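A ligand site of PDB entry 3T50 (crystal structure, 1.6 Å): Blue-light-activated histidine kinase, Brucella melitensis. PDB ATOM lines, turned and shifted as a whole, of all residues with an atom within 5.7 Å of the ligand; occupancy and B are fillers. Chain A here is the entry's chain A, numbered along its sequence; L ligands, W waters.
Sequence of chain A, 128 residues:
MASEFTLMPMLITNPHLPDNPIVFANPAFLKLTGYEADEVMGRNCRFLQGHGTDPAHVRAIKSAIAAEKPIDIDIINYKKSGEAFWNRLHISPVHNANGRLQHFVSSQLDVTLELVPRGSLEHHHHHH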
ATOM      1  N   LEU A  11     -15.310  -3.828   9.410  1.00  0.00           N
ATOM      2  CA  LEU A  11     -15.056  -4.884  10.428  1.00  0.00           C
ATOM      3  C   LEU A  11     -15.098  -6.209   9.764  1.00  0.00           C
ATOM      4  O   LEU A  11     -15.817  -6.382   8.762  1.00  0.00           O
ATOM      5  CB  LEU A  11     -16.156  -4.895  11.477  1.00  0.00           C
ATOM      6  CG  LEU A  11     -16.325  -3.662  12.335  1.00  0.00           C
ATOM      7  CD1 LEU A  11     -17.453  -3.883  13.332  1.00  0.00           C
ATOM      8  CD2 LEU A  11     -15.018  -3.361  13.140  1.00  0.00           C
ATOM      9  N   ILE A  12     -14.356  -7.161  10.312  1.00  0.00           N
ATOM     10  CA  ILE A  12     -14.601  -8.584   9.965  1.00  0.00           C
ATOM     11  C   ILE A  12     -14.855  -9.304  11.286  1.00  0.00           C
ATOM     12  O   ILE A  12     -14.145  -9.081  12.287  1.00  0.00           O
ATOM     13  CB  ILE A  12     -13.368  -9.211   9.257  1.00  0.00           C
ATOM     14  CG1 ILE A  12     -13.095  -8.509   7.912  1.00  0.00           C
ATOM     15  CG2 ILE A  12     -13.580 -10.707   9.000  1.00  0.00           C
ATOM     16  CD1 ILE A  12     -11.755  -8.829   7.355  1.00  0.00           C
ATOM     17  N   THR A  13     -15.867 -10.161  11.274  1.00  0.00           N
ATOM     18  CA  THR A  13     -16.148 -11.011  12.426  1.00  0.00           C
ATOM     19  C   THR A  13     -16.011 -12.490  12.072  1.00  0.00           C
ATOM     20  O   THR A  13     -16.040 -12.872  10.883  1.00  0.00           O
ATOM     21  CB  THR A  13     -17.567 -10.818  12.956  1.00  0.00           C
ATOM     22  OG1 THR A  13     -18.533 -11.327  12.030  1.00  0.00           O
ATOM     23  CG2 THR A  13     -17.827  -9.332  13.275  1.00  0.00           C
ATOM     24  N   ASP A  19     -20.428 -16.046  19.810  1.00  0.00           N
ATOM     25  CA  ASP A  19     -20.901 -14.647  19.770  1.00  0.00           C
ATOM     26  C   ASP A  19     -20.288 -13.830  18.641  1.00  0.00           C
ATOM     27  O   ASP A  19     -20.406 -12.602  18.618  1.00  0.00           O
ATOM     28  CB  ASP A  19     -20.758 -13.956  21.140  1.00  0.00           C
ATOM     29  CG  ASP A  19     -21.805 -12.873  21.358  1.00  0.00           C
ATOM     30  OD1 ASP A  19     -22.821 -12.867  20.644  1.00  0.00           O
ATOM     31  OD2 ASP A  19     -21.527 -11.990  22.183  1.00  0.00           O
ATOM     32  N   ASN A  20     -19.791 -14.522  17.615  1.00  0.00           N
ATOM     33  CA  ASN A  20     -19.418 -13.832  16.341  1.00  0.00           C
ATOM     34  C   ASN A  20     -18.570 -12.571  16.568  1.00  0.00           C
ATOM     35  O   ASN A  20     -18.937 -11.448  16.154  1.00  0.00           O
ATOM     36  CB  ASN A  20     -20.692 -13.517  15.540  1.00  0.00           C
ATOM     37  CG  ASN A  20     -20.428 -13.134  14.105  1.00  0.00           C
ATOM     38  OD1 ASN A  20     -19.431 -13.484  13.522  1.00  0.00           O
ATOM     39  ND2 ASN A  20     -21.339 -12.343  13.564  1.00  0.00           N
ATOM     40  N   PHE A  29     -12.483   2.519  11.092  1.00  0.00           N
ATOM     41  CA  PHE A  29     -13.543   2.218  12.059  1.00  0.00           C
ATOM     42  C   PHE A  29     -13.162   2.749  13.439  1.00  0.00           C
ATOM     43  O   PHE A  29     -14.008   3.271  14.172  1.00  0.00           O
ATOM     44  CB  PHE A  29     -13.800   0.712  12.099  1.00  0.00           C
ATOM     45  CG  PHE A  29     -14.768   0.287  13.146  1.00  0.00           C
ATOM     46  CD1 PHE A  29     -16.136   0.111  12.849  1.00  0.00           C
ATOM     47  CD2 PHE A  29     -14.301   0.090  14.463  1.00  0.00           C
ATOM     48  CE1 PHE A  29     -17.013  -0.288  13.864  1.00  0.00           C
ATOM     49  CE2 PHE A  29     -15.155  -0.306  15.483  1.00  0.00           C
ATOM     50  CZ  PHE A  29     -16.519  -0.522  15.177  1.00  0.00           C
ATOM     51  N   ASN A  44     -18.489  -8.913  20.229  1.00  0.00           N
ATOM     52  CA  ASN A  44     -19.583  -8.733  19.296  1.00  0.00           C
ATOM     53  C   ASN A  44     -19.834  -7.238  19.119  1.00  0.00           C
ATOM     54  O   ASN A  44     -19.733  -6.484  20.074  1.00  0.00           O
ATOM     55  CB  ASN A  44     -20.835  -9.393  19.886  1.00  0.00           C
ATOM     56  CG  ASN A  44     -21.980  -9.406  18.905  1.00  0.00           C
ATOM     57  OD1 ASN A  44     -22.660  -8.382  18.729  1.00  0.00           O
ATOM     58  ND2 ASN A  44     -22.175 -10.535  18.220  1.00  0.00           N
ATOM     59  N   CYS A  45     -20.170  -6.833  17.895  1.00  0.00           N
ATOM     60  CA  CYS A  45     -20.267  -5.417  17.557  1.00  0.00           C
ATOM     61  C   CYS A  45     -21.346  -4.710  18.360  1.00  0.00           C
ATOM     62  O   CYS A  45     -21.293  -3.489  18.495  1.00  0.00           O
ATOM     63  CB  CYS A  45     -20.507  -5.255  16.071  1.00  0.00           C
ATOM     64  SG  CYS A  45     -20.147  -3.584  15.464  1.00  0.00           S
ATOM     65  N   ARG A  46     -22.327  -5.456  18.887  1.00  0.00           N
ATOM     66  CA  ARG A  46     -23.441  -4.828  19.621  1.00  0.00           C
ATOM     67  C   ARG A  46     -23.040  -3.825  20.709  1.00  0.00           C
ATOM     68  O   ARG A  46     -23.926  -3.063  21.169  1.00  0.00           O
ATOM     69  CB  ARG A  46     -24.399  -5.863  20.213  1.00  0.00           C
ATOM     70  CG  ARG A  46     -23.805  -6.538  21.461  1.00  0.00           C
ATOM     71  CD  ARG A  46     -24.885  -7.387  22.160  1.00  0.00           C
ATOM     72  NE  ARG A  46     -25.167  -8.595  21.397  1.00  0.00           N
ATOM     73  CZ  ARG A  46     -24.372  -9.674  21.398  1.00  0.00           C
ATOM     74  NH1 ARG A  46     -23.295  -9.730  22.163  1.00  0.00           N
ATOM     75  NH2 ARG A  46     -24.706 -10.728  20.657  1.00  0.00           N
ATOM     76  N   LEU A  48     -21.631  -1.232  20.369  1.00  0.00           N
ATOM     77  CA  LEU A  48     -21.867   0.082  19.802  1.00  0.00           C
ATOM     78  C   LEU A  48     -23.299   0.601  20.058  1.00  0.00           C
ATOM     79  O   LEU A  48     -23.549   1.790  19.840  1.00  0.00           O
ATOM     80  CB  LEU A  48     -21.588   0.079  18.286  1.00  0.00           C
ATOM     81  CG  LEU A  48     -20.104  -0.068  17.892  1.00  0.00           C
ATOM     82  CD1 LEU A  48     -20.106  -0.172  16.341  1.00  0.00           C
ATOM     83  CD2 LEU A  48     -19.332   1.145  18.344  1.00  0.00           C
ATOM     84  N   GLN A  49     -24.224  -0.240  20.487  1.00  0.00           N
ATOM     85  CA  GLN A  49     -25.618   0.150  20.630  1.00  0.00           C
ATOM     86  C   GLN A  49     -25.838   0.789  22.010  1.00  0.00           C
ATOM     87  O   GLN A  49     -24.974   0.680  22.896  1.00  0.00           O
ATOM     88  CB  GLN A  49     -26.499  -1.095  20.450  1.00  0.00           C
ATOM     89  CG  GLN A  49     -26.404  -1.695  19.054  1.00  0.00           C
ATOM     90  CD  GLN A  49     -26.887  -3.132  18.975  1.00  0.00           C
ATOM     91  OE1 GLN A  49     -27.501  -3.650  19.911  1.00  0.00           O
ATOM     92  NE2 GLN A  49     -26.596  -3.802  17.838  1.00  0.00           N
ATOM     93  N   THR A  53     -30.920   3.090  20.469  1.00  0.00           N
ATOM     94  CA  THR A  53     -30.928   2.124  19.355  1.00  0.00           C
ATOM     95  C   THR A  53     -32.291   1.448  19.304  1.00  0.00           C
ATOM     96  O   THR A  53     -32.759   0.948  20.350  1.00  0.00           O
ATOM     97  CB  THR A  53     -29.859   1.037  19.594  1.00  0.00           C
ATOM     98  OG1 THR A  53     -28.579   1.692  19.766  1.00  0.00           O
ATOM     99  CG2 THR A  53     -29.838   0.055  18.412  1.00  0.00           C
ATOM    100  N   VAL A  58     -32.061  -3.906  15.481  1.00  0.00           N
ATOM    101  CA  VAL A  58     -31.223  -4.944  16.023  1.00  0.00           C
ATOM    102  C   VAL A  58     -31.785  -6.302  15.607  1.00  0.00           C
ATOM    103  O   VAL A  58     -31.056  -7.182  15.148  1.00  0.00           O
ATOM    104  CB  VAL A  58     -31.167  -4.851  17.573  1.00  0.00           C
ATOM    105  CG1 VAL A  58     -30.431  -6.067  18.169  1.00  0.00           C
ATOM    106  CG2 VAL A  58     -30.523  -3.559  18.026  1.00  0.00           C
ATOM    107  N   ARG A  59     -33.089  -6.474  15.778  1.00  0.00           N
ATOM    108  CA  ARG A  59     -33.725  -7.725  15.299  1.00  0.00           C
ATOM    109  C   ARG A  59     -33.597  -7.958  13.769  1.00  0.00           C
ATOM    110  O   ARG A  59     -33.418  -9.106  13.344  1.00  0.00           O
ATOM    111  CB  ARG A  59     -35.199  -7.768  15.734  1.00  0.00           C
ATOM    112  CG  ARG A  59     -35.411  -7.794  17.248  1.00  0.00           C
ATOM    113  CD  ARG A  59     -36.892  -8.042  17.635  1.00  0.00           C
ATOM    114  NE  ARG A  59     -37.776  -7.056  16.994  1.00  0.00           N
ATOM    115  CZ  ARG A  59     -38.295  -5.993  17.601  1.00  0.00           C
ATOM    116  NH1 ARG A  59     -38.042  -5.761  18.884  1.00  0.00           N
ATOM    117  NH2 ARG A  59     -39.067  -5.171  16.915  1.00  0.00           N
ATOM    118  N   ILE A  61     -31.116  -6.997  11.909  1.00  0.00           N
ATOM    119  CA  ILE A  61     -29.710  -7.417  11.704  1.00  0.00           C
ATOM    120  C   ILE A  61     -29.559  -8.862  12.123  1.00  0.00           C
ATOM    121  O   ILE A  61     -28.980  -9.644  11.393  1.00  0.00           O
ATOM    122  CB  ILE A  61     -28.714  -6.491  12.474  1.00  0.00           C
ATOM    123  CG1 ILE A  61     -28.783  -5.077  11.894  1.00  0.00           C
ATOM    124  CG2 ILE A  61     -27.272  -7.034  12.381  1.00  0.00           C
ATOM    125  CD1 ILE A  61     -28.171  -4.020  12.852  1.00  0.00           C
ATOM    126  N   LYS A  62     -30.069  -9.223  13.313  1.00  0.00           N
ATOM    127  CA  LYS A  62     -29.942 -10.568  13.835  1.00  0.00           C
ATOM    128  C   LYS A  62     -30.572 -11.528  12.823  1.00  0.00           C
ATOM    129  O   LYS A  62     -30.022 -12.576  12.547  1.00  0.00           O
ATOM    130  CB  LYS A  62     -30.648 -10.736  15.177  1.00  0.00           C
ATOM    131  CG  LYS A  62     -30.212 -12.010  15.924  1.00  0.00           C
ATOM    132  CD  LYS A  62     -31.379 -12.735  16.562  1.00  0.00           C
ATOM    133  CE  LYS A  62     -31.588 -12.366  18.019  1.00  0.00           C
ATOM    134  NZ  LYS A  62     -32.705 -13.152  18.691  1.00  0.00           N
ATOM    135  N   ILE A  65     -28.326 -11.883   9.592  1.00  0.00           N
ATOM    136  CA  ILE A  65     -27.150 -12.663   9.983  1.00  0.00           C
ATOM    137  C   ILE A  65     -27.523 -14.136  10.088  1.00  0.00           C
ATOM    138  O   ILE A  65     -26.809 -14.990   9.578  1.00  0.00           O
ATOM    139  CB  ILE A  65     -26.494 -12.107  11.271  1.00  0.00           C
ATOM    140  CG1 ILE A  65     -25.828 -10.752  10.906  1.00  0.00           C
ATOM    141  CG2 ILE A  65     -25.506 -13.095  11.911  1.00  0.00           C
ATOM    142  CD1 ILE A  65     -25.352  -9.977  12.064  1.00  0.00           C
ATOM    143  N   ILE A  75     -28.630   2.623  11.730  1.00  0.00           N
ATOM    144  CA  ILE A  75     -28.872   2.303  13.126  1.00  0.00           C
ATOM    145  C   ILE A  75     -28.179   3.353  14.025  1.00  0.00           C
ATOM    146  O   ILE A  75     -27.105   3.847  13.720  1.00  0.00           O
ATOM    147  CB  ILE A  75     -28.385   0.854  13.463  1.00  0.00           C
ATOM    148  CG1 ILE A  75     -28.826   0.409  14.849  1.00  0.00           C
ATOM    149  CG2 ILE A  75     -26.798   0.763  13.382  1.00  0.00           C
ATOM    150  CD1 ILE A  75     -28.600  -1.064  15.254  1.00  0.00           C
ATOM    151  N   ILE A  76     -28.810   3.689  15.155  1.00  0.00           N
ATOM    152  CA  ILE A  76     -28.156   4.582  16.135  1.00  0.00           C
ATOM    153  C   ILE A  76     -27.108   3.842  16.950  1.00  0.00           C
ATOM    154  O   ILE A  76     -27.386   2.785  17.551  1.00  0.00           O
ATOM    155  CB  ILE A  76     -29.216   5.245  17.080  1.00  0.00           C
ATOM    156  CG1 ILE A  76     -30.099   6.207  16.286  1.00  0.00           C
ATOM    157  CG2 ILE A  76     -28.492   5.932  18.262  1.00  0.00           C
ATOM    158  CD1 ILE A  76     -31.289   6.763  17.132  1.00  0.00           C
ATOM    159  N   ASN A  77     -25.901   4.378  16.941  1.00  0.00           N
ATOM    160  CA  ASN A  77     -24.769   3.792  17.647  1.00  0.00           C
ATOM    161  C   ASN A  77     -24.094   4.916  18.432  1.00  0.00           C
ATOM    162  O   ASN A  77     -24.470   6.108  18.344  1.00  0.00           O
ATOM    163  CB  ASN A  77     -23.758   3.191  16.667  1.00  0.00           C
ATOM    164  CG  ASN A  77     -24.091   1.740  16.229  1.00  0.00           C
ATOM    165  OD1 ASN A  77     -23.367   1.194  15.400  1.00  0.00           O
ATOM    166  ND2 ASN A  77     -25.173   1.119  16.770  1.00  0.00           N
ATOM    167  N   ASN A  87     -25.263   5.293  12.151  1.00  0.00           N
ATOM    168  CA  ASN A  87     -24.290   4.440  11.503  1.00  0.00           C
ATOM    169  C   ASN A  87     -25.015   3.704  10.375  1.00  0.00           C
ATOM    170  O   ASN A  87     -25.943   2.930  10.657  1.00  0.00           O
ATOM    171  CB  ASN A  87     -23.772   3.431  12.533  1.00  0.00           C
ATOM    172  CG  ASN A  87     -22.641   2.548  12.007  1.00  0.00           C
ATOM    173  OD1 ASN A  87     -22.153   2.715  10.896  1.00  0.00           O
ATOM    174  ND2 ASN A  87     -22.211   1.610  12.837  1.00  0.00           N
ATOM    175  N   LEU A  89     -24.876   0.863   8.059  1.00  0.00           N
ATOM    176  CA  LEU A  89     -24.221  -0.399   8.225  1.00  0.00           C
ATOM    177  C   LEU A  89     -24.495  -1.213   6.963  1.00  0.00           C
ATOM    178  O   LEU A  89     -25.639  -1.302   6.530  1.00  0.00           O
ATOM    179  CB  LEU A  89     -24.817  -1.038   9.472  1.00  0.00           C
ATOM    180  CG  LEU A  89     -24.402  -2.351  10.051  1.00  0.00           C
ATOM    181  CD1 LEU A  89     -22.858  -2.432  10.245  1.00  0.00           C
ATOM    182  CD2 LEU A  89     -25.097  -2.385  11.404  1.00  0.00           C
ATOM    183  N   ILE A  91     -23.729  -5.086   6.003  1.00  0.00           N
ATOM    184  CA  ILE A  91     -23.151  -6.343   6.472  1.00  0.00           C
ATOM    185  C   ILE A  91     -23.360  -7.384   5.375  1.00  0.00           C
ATOM    186  O   ILE A  91     -24.471  -7.491   4.844  1.00  0.00           O
ATOM    187  CB  ILE A  91     -23.835  -6.813   7.778  1.00  0.00           C
ATOM    188  CG1 ILE A  91     -23.536  -5.796   8.888  1.00  0.00           C
ATOM    189  CG2 ILE A  91     -23.310  -8.201   8.237  1.00  0.00           C
ATOM    190  CD1 ILE A  91     -24.489  -5.880  10.074  1.00  0.00           C
ATOM    191  N   PHE A 104     -18.112 -12.801   8.497  1.00  0.00           N
ATOM    192  CA  PHE A 104     -18.927 -11.666   8.036  1.00  0.00           C
ATOM    193  C   PHE A 104     -18.025 -10.437   7.884  1.00  0.00           C
ATOM    194  O   PHE A 104     -17.030 -10.304   8.613  1.00  0.00           O
ATOM    195  CB  PHE A 104     -20.045 -11.297   9.013  1.00  0.00           C
ATOM    196  CG  PHE A 104     -21.162 -12.313   9.064  1.00  0.00           C
ATOM    197  CD1 PHE A 104     -22.258 -12.192   8.217  1.00  0.00           C
ATOM    198  CD2 PHE A 104     -21.088 -13.382   9.968  1.00  0.00           C
ATOM    199  CE1 PHE A 104     -23.312 -13.167   8.252  1.00  0.00           C
ATOM    200  CE2 PHE A 104     -22.090 -14.358  10.003  1.00  0.00           C
ATOM    201  CZ  PHE A 104     -23.194 -14.228   9.177  1.00  0.00           C
ATOM    202  N   VAL A 105     -18.381  -9.569   6.961  1.00  0.00           N
ATOM    203  CA  VAL A 105     -17.673  -8.314   6.757  1.00  0.00           C
ATOM    204  C   VAL A 105     -18.683  -7.181   6.718  1.00  0.00           C
ATOM    205  O   VAL A 105     -19.875  -7.369   6.363  1.00  0.00           O
ATOM    206  CB  VAL A 105     -16.819  -8.363   5.448  1.00  0.00           C
ATOM    207  CG1 VAL A 105     -17.680  -8.475   4.227  1.00  0.00           C
ATOM    208  CG2 VAL A 105     -15.897  -7.148   5.374  1.00  0.00           C
ATOM    209  N   SER A 106     -18.253  -5.998   7.153  1.00  0.00           N
ATOM    210  CA  SER A 106     -19.137  -4.823   7.104  1.00  0.00           C
ATOM    211  C   SER A 106     -18.423  -3.585   6.592  1.00  0.00           C
ATOM    212  O   SER A 106     -17.191  -3.500   6.679  1.00  0.00           O
ATOM    213  CB  SER A 106     -19.695  -4.496   8.505  1.00  0.00           C
ATOM    214  OG  SER A 106     -18.620  -4.214   9.372  1.00  0.00           O
ATOM    215  N   GLN A 108     -19.106   0.666   7.469  1.00  0.00           N
ATOM    216  CA  GLN A 108     -19.810   1.543   8.405  1.00  0.00           C
ATOM    217  C   GLN A 108     -19.522   2.951   7.923  1.00  0.00           C
ATOM    218  O   GLN A 108     -18.493   3.226   7.303  1.00  0.00           O
ATOM    219  CB  GLN A 108     -19.375   1.374   9.870  1.00  0.00           C
ATOM    220  CG  GLN A 108     -19.981   0.152  10.644  1.00  0.00           C
ATOM    221  CD  GLN A 108     -19.250  -1.157  10.468  1.00  0.00           C
ATOM    222  OE1 GLN A 108     -18.335  -1.294   9.633  1.00  0.00           O
ATOM    223  NE2 GLN A 108     -19.648  -2.129  11.243  1.00  0.00           N
HETATM  224  N1  LIG L   1     -24.283  -3.725  15.179  1.00  0.00           N
HETATM  225  C1  LIG L   1     -24.224  -2.367  15.437  1.00  0.00           C
HETATM  226  O1  LIG L   1     -25.011  -1.864  16.190  1.00  0.00           O
HETATM  227  N2  LIG L   1     -23.268  -1.567  14.840  1.00  0.00           N
HETATM  228  C2  LIG L   1     -22.346  -2.069  13.955  1.00  0.00           C
HETATM  229  O2  LIG L   1     -21.523  -1.288  13.491  1.00  0.00           O
HETATM  230  C3  LIG L   1     -22.393  -3.435  13.696  1.00  0.00           C
HETATM  231  N3  LIG L   1     -21.483  -3.991  12.807  1.00  0.00           N
HETATM  232  C4  LIG L   1     -21.574  -5.334  12.555  1.00  0.00           C
HETATM  233  C5  LIG L   1     -20.662  -5.859  11.653  1.00  0.00           C
HETATM  234  C6  LIG L   1     -20.709  -7.225  11.393  1.00  0.00           C
HETATM  235  C7  LIG L   1     -19.709  -7.818  10.416  1.00  0.00           C
HETATM  236  C8  LIG L   1     -21.667  -8.046  12.013  1.00  0.00           C
HETATM  237  C9  LIG L   1     -21.726  -9.537  11.702  1.00  0.00           C
HETATM  238  C10 LIG L   1     -22.600  -7.514  12.919  1.00  0.00           C
HETATM  239  C11 LIG L   1     -22.543  -6.136  13.186  1.00  0.00           C
HETATM  240  N4  LIG L   1     -23.451  -5.579  14.084  1.00  0.00           N
HETATM  241  C12 LIG L   1     -23.352  -4.225  14.334  1.00  0.00           C
HETATM  242  C13 LIG L   1     -24.569  -6.346  14.725  1.00  0.00           C
HETATM  243  C14 LIG L   1     -24.360  -6.994  16.075  1.00  0.00           C
HETATM  244  O3  LIG L   1     -23.096  -7.617  16.057  1.00  0.00           O
HETATM  245  C15 LIG L   1     -25.481  -8.058  16.253  1.00  0.00           C
HETATM  246  O4  LIG L   1     -25.497  -8.945  15.115  1.00  0.00           O
HETATM  247  C16 LIG L   1     -26.860  -7.432  16.367  1.00  0.00           C
HETATM  248  O5  LIG L   1     -26.875  -6.621  17.538  1.00  0.00           O
HETATM  249  C17 LIG L   1     -27.991  -8.502  16.405  1.00  0.00           C
HETATM  250  O6  LIG L   1     -27.680  -9.519  17.337  1.00  0.00           O
HETATM  251  P1  LIG L   1     -27.999  -9.522  18.903  1.00  0.00           P
HETATM  252  O7  LIG L   1     -29.519  -9.499  19.046  1.00  0.00           O
HETATM  253  O8  LIG L   1     -27.378 -10.759  19.484  1.00  0.00           O
HETATM  254  O9  LIG L   1     -27.420  -8.286  19.579  1.00  0.00           O
HETATM  255  O   HOH W   1     -20.405  -9.090  15.919  1.00  0.00           O
HETATM  256  O   HOH W   2     -23.587 -11.192  15.452  1.00  0.00           O
HETATM  257  O   HOH W   3     -26.587 -11.573  15.460  1.00  0.00           O
HETATM  258  O   HOH W   4     -26.465 -12.692  17.956  1.00  0.00           O
HETATM  259  O   HOH W   5     -28.196  -6.028  20.943  1.00  0.00           O
HETATM  260  O   HOH W   6     -32.173  -8.986  18.357  1.00  0.00           O
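OG1 of Thr 13 touches C9 of the ligand, at 3.7 Å.
Asn 20 touches the ligand (ND2 to C9, 3.4 Å).
Leu 48 touches the ligand (CD1 to O2, 3.4 Å).
Val 58 touches the ligand (O to C17, 3.6 Å).
Ile 61 touches the ligand.
CE of Lys 62 touches O7 of the ligand, 3.7 Å away.
CD1 of Ile 65 touches O4 of the ligand (3.2 Å).
Ile 75 touches the ligand.
Leu 89 touches the ligand (CD1 to N3, 3.3 Å).
Ile 91 touches the ligand.
Phe 104 touches the ligand (CB to C9, 3.6 Å).
C of Val 105 touches C7 of the ligand, 3.9 Å away.
Ser 106 touches the ligand.
Hydrophobic or aromatic side chains that line the ligand: Leu 48, Val 58, Ile 61, Ile 65, Ile 75, Leu 89, Ile 91 and Phe 104.
Within 4 Å of the ligand: Thr 13, Asn 20, Asn 44, Cys 45, Arg 46, Leu 48, Gln 49, Val 58, Ile 61, Lys 62, Ile 65, Ile 75, Asn 77, Asn 87, Leu 89, Ile 91, Phe 104, Val 105, Ser 106 and Gln 108.
The nearest printed residue that does not touch the ligand is Leu 11 (4.1 Å).
The side-chain amide oxygen of Asn 44 is in hydrogen-bond range of an oxygen (O3) of the ligand (2.8 Å).
The side-chain amide oxygen (OD1) of Asn 77 is in hydrogen-bond range of a nitrogen (N2) of the ligand, 2.8 Å away.
O5 of the ligand lies within hydrogen-bond range of NE2 of Gln 49.
SG of Cys 45 lies close to N3 of the ligand (3.0 Å).
NE of Arg 46 lies within salt-bridge range of O9 of the ligand (2.9 Å).
NE2 of Gln 108 sits at hydrogen-bond distance from O2 of the ligand (3.0 Å).
ND2 of Asn 87 lies within hydrogen-bond range of O2 of the ligand, at 3.0 Å.
Water W5 bridges OE1 of Gln 49 (2.7 Å) and O9 of the ligand (2.7 Å).
Water W2 lies within hydrogen-bond range of an oxygen (O4) of the ligand (3.0 Å), the side-chain amide nitrogen of Asn 20 (3.2 Å) and the side-chain amide nitrogen of Asn 44 (3.2 Å).
Water W1 lies within hydrogen-bond range of O of Asn 20, N of Cys 45, O3 of the ligand and ND2 of Asn 44.
The side-chain amide oxygen of Asn 44 is in hydrogen-bond range of the backbone NH of Arg 46 (2.9 Å).
ND2 of Asn 44 is in hydrogen-bond range of O of Asp 19, at 2.7 Å.
The side-chain amide oxygen (OD1) of Asn 77 is in hydrogen-bond range of the side-chain amide nitrogen (ND2) of Asn 87 (2.8 Å).
The side-chain carboxylate (OD1) of Asp 19 is in salt-bridge range of the guanidinium group (NH2) of Arg 46 (2.9 Å).
The backbone NH of Asn 87 lies within hydrogen-bond range of the backbone carbonyl oxygen of Ile 75, at 2.8 Å.
The side-chain hydroxyl (OG1) of Thr 13 lies within hydrogen-bond range of the side-chain amide oxygen (OD1) of Asn 20, 2.8 Å away.
N of Ser 106 lies within hydrogen-bond range of O of Leu 11, at 2.9 Å.
The backbone carbonyl oxygen (O) of Phe 104 is in hydrogen-bond range of the backbone NH (N) of Thr 13 (2.9 Å).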
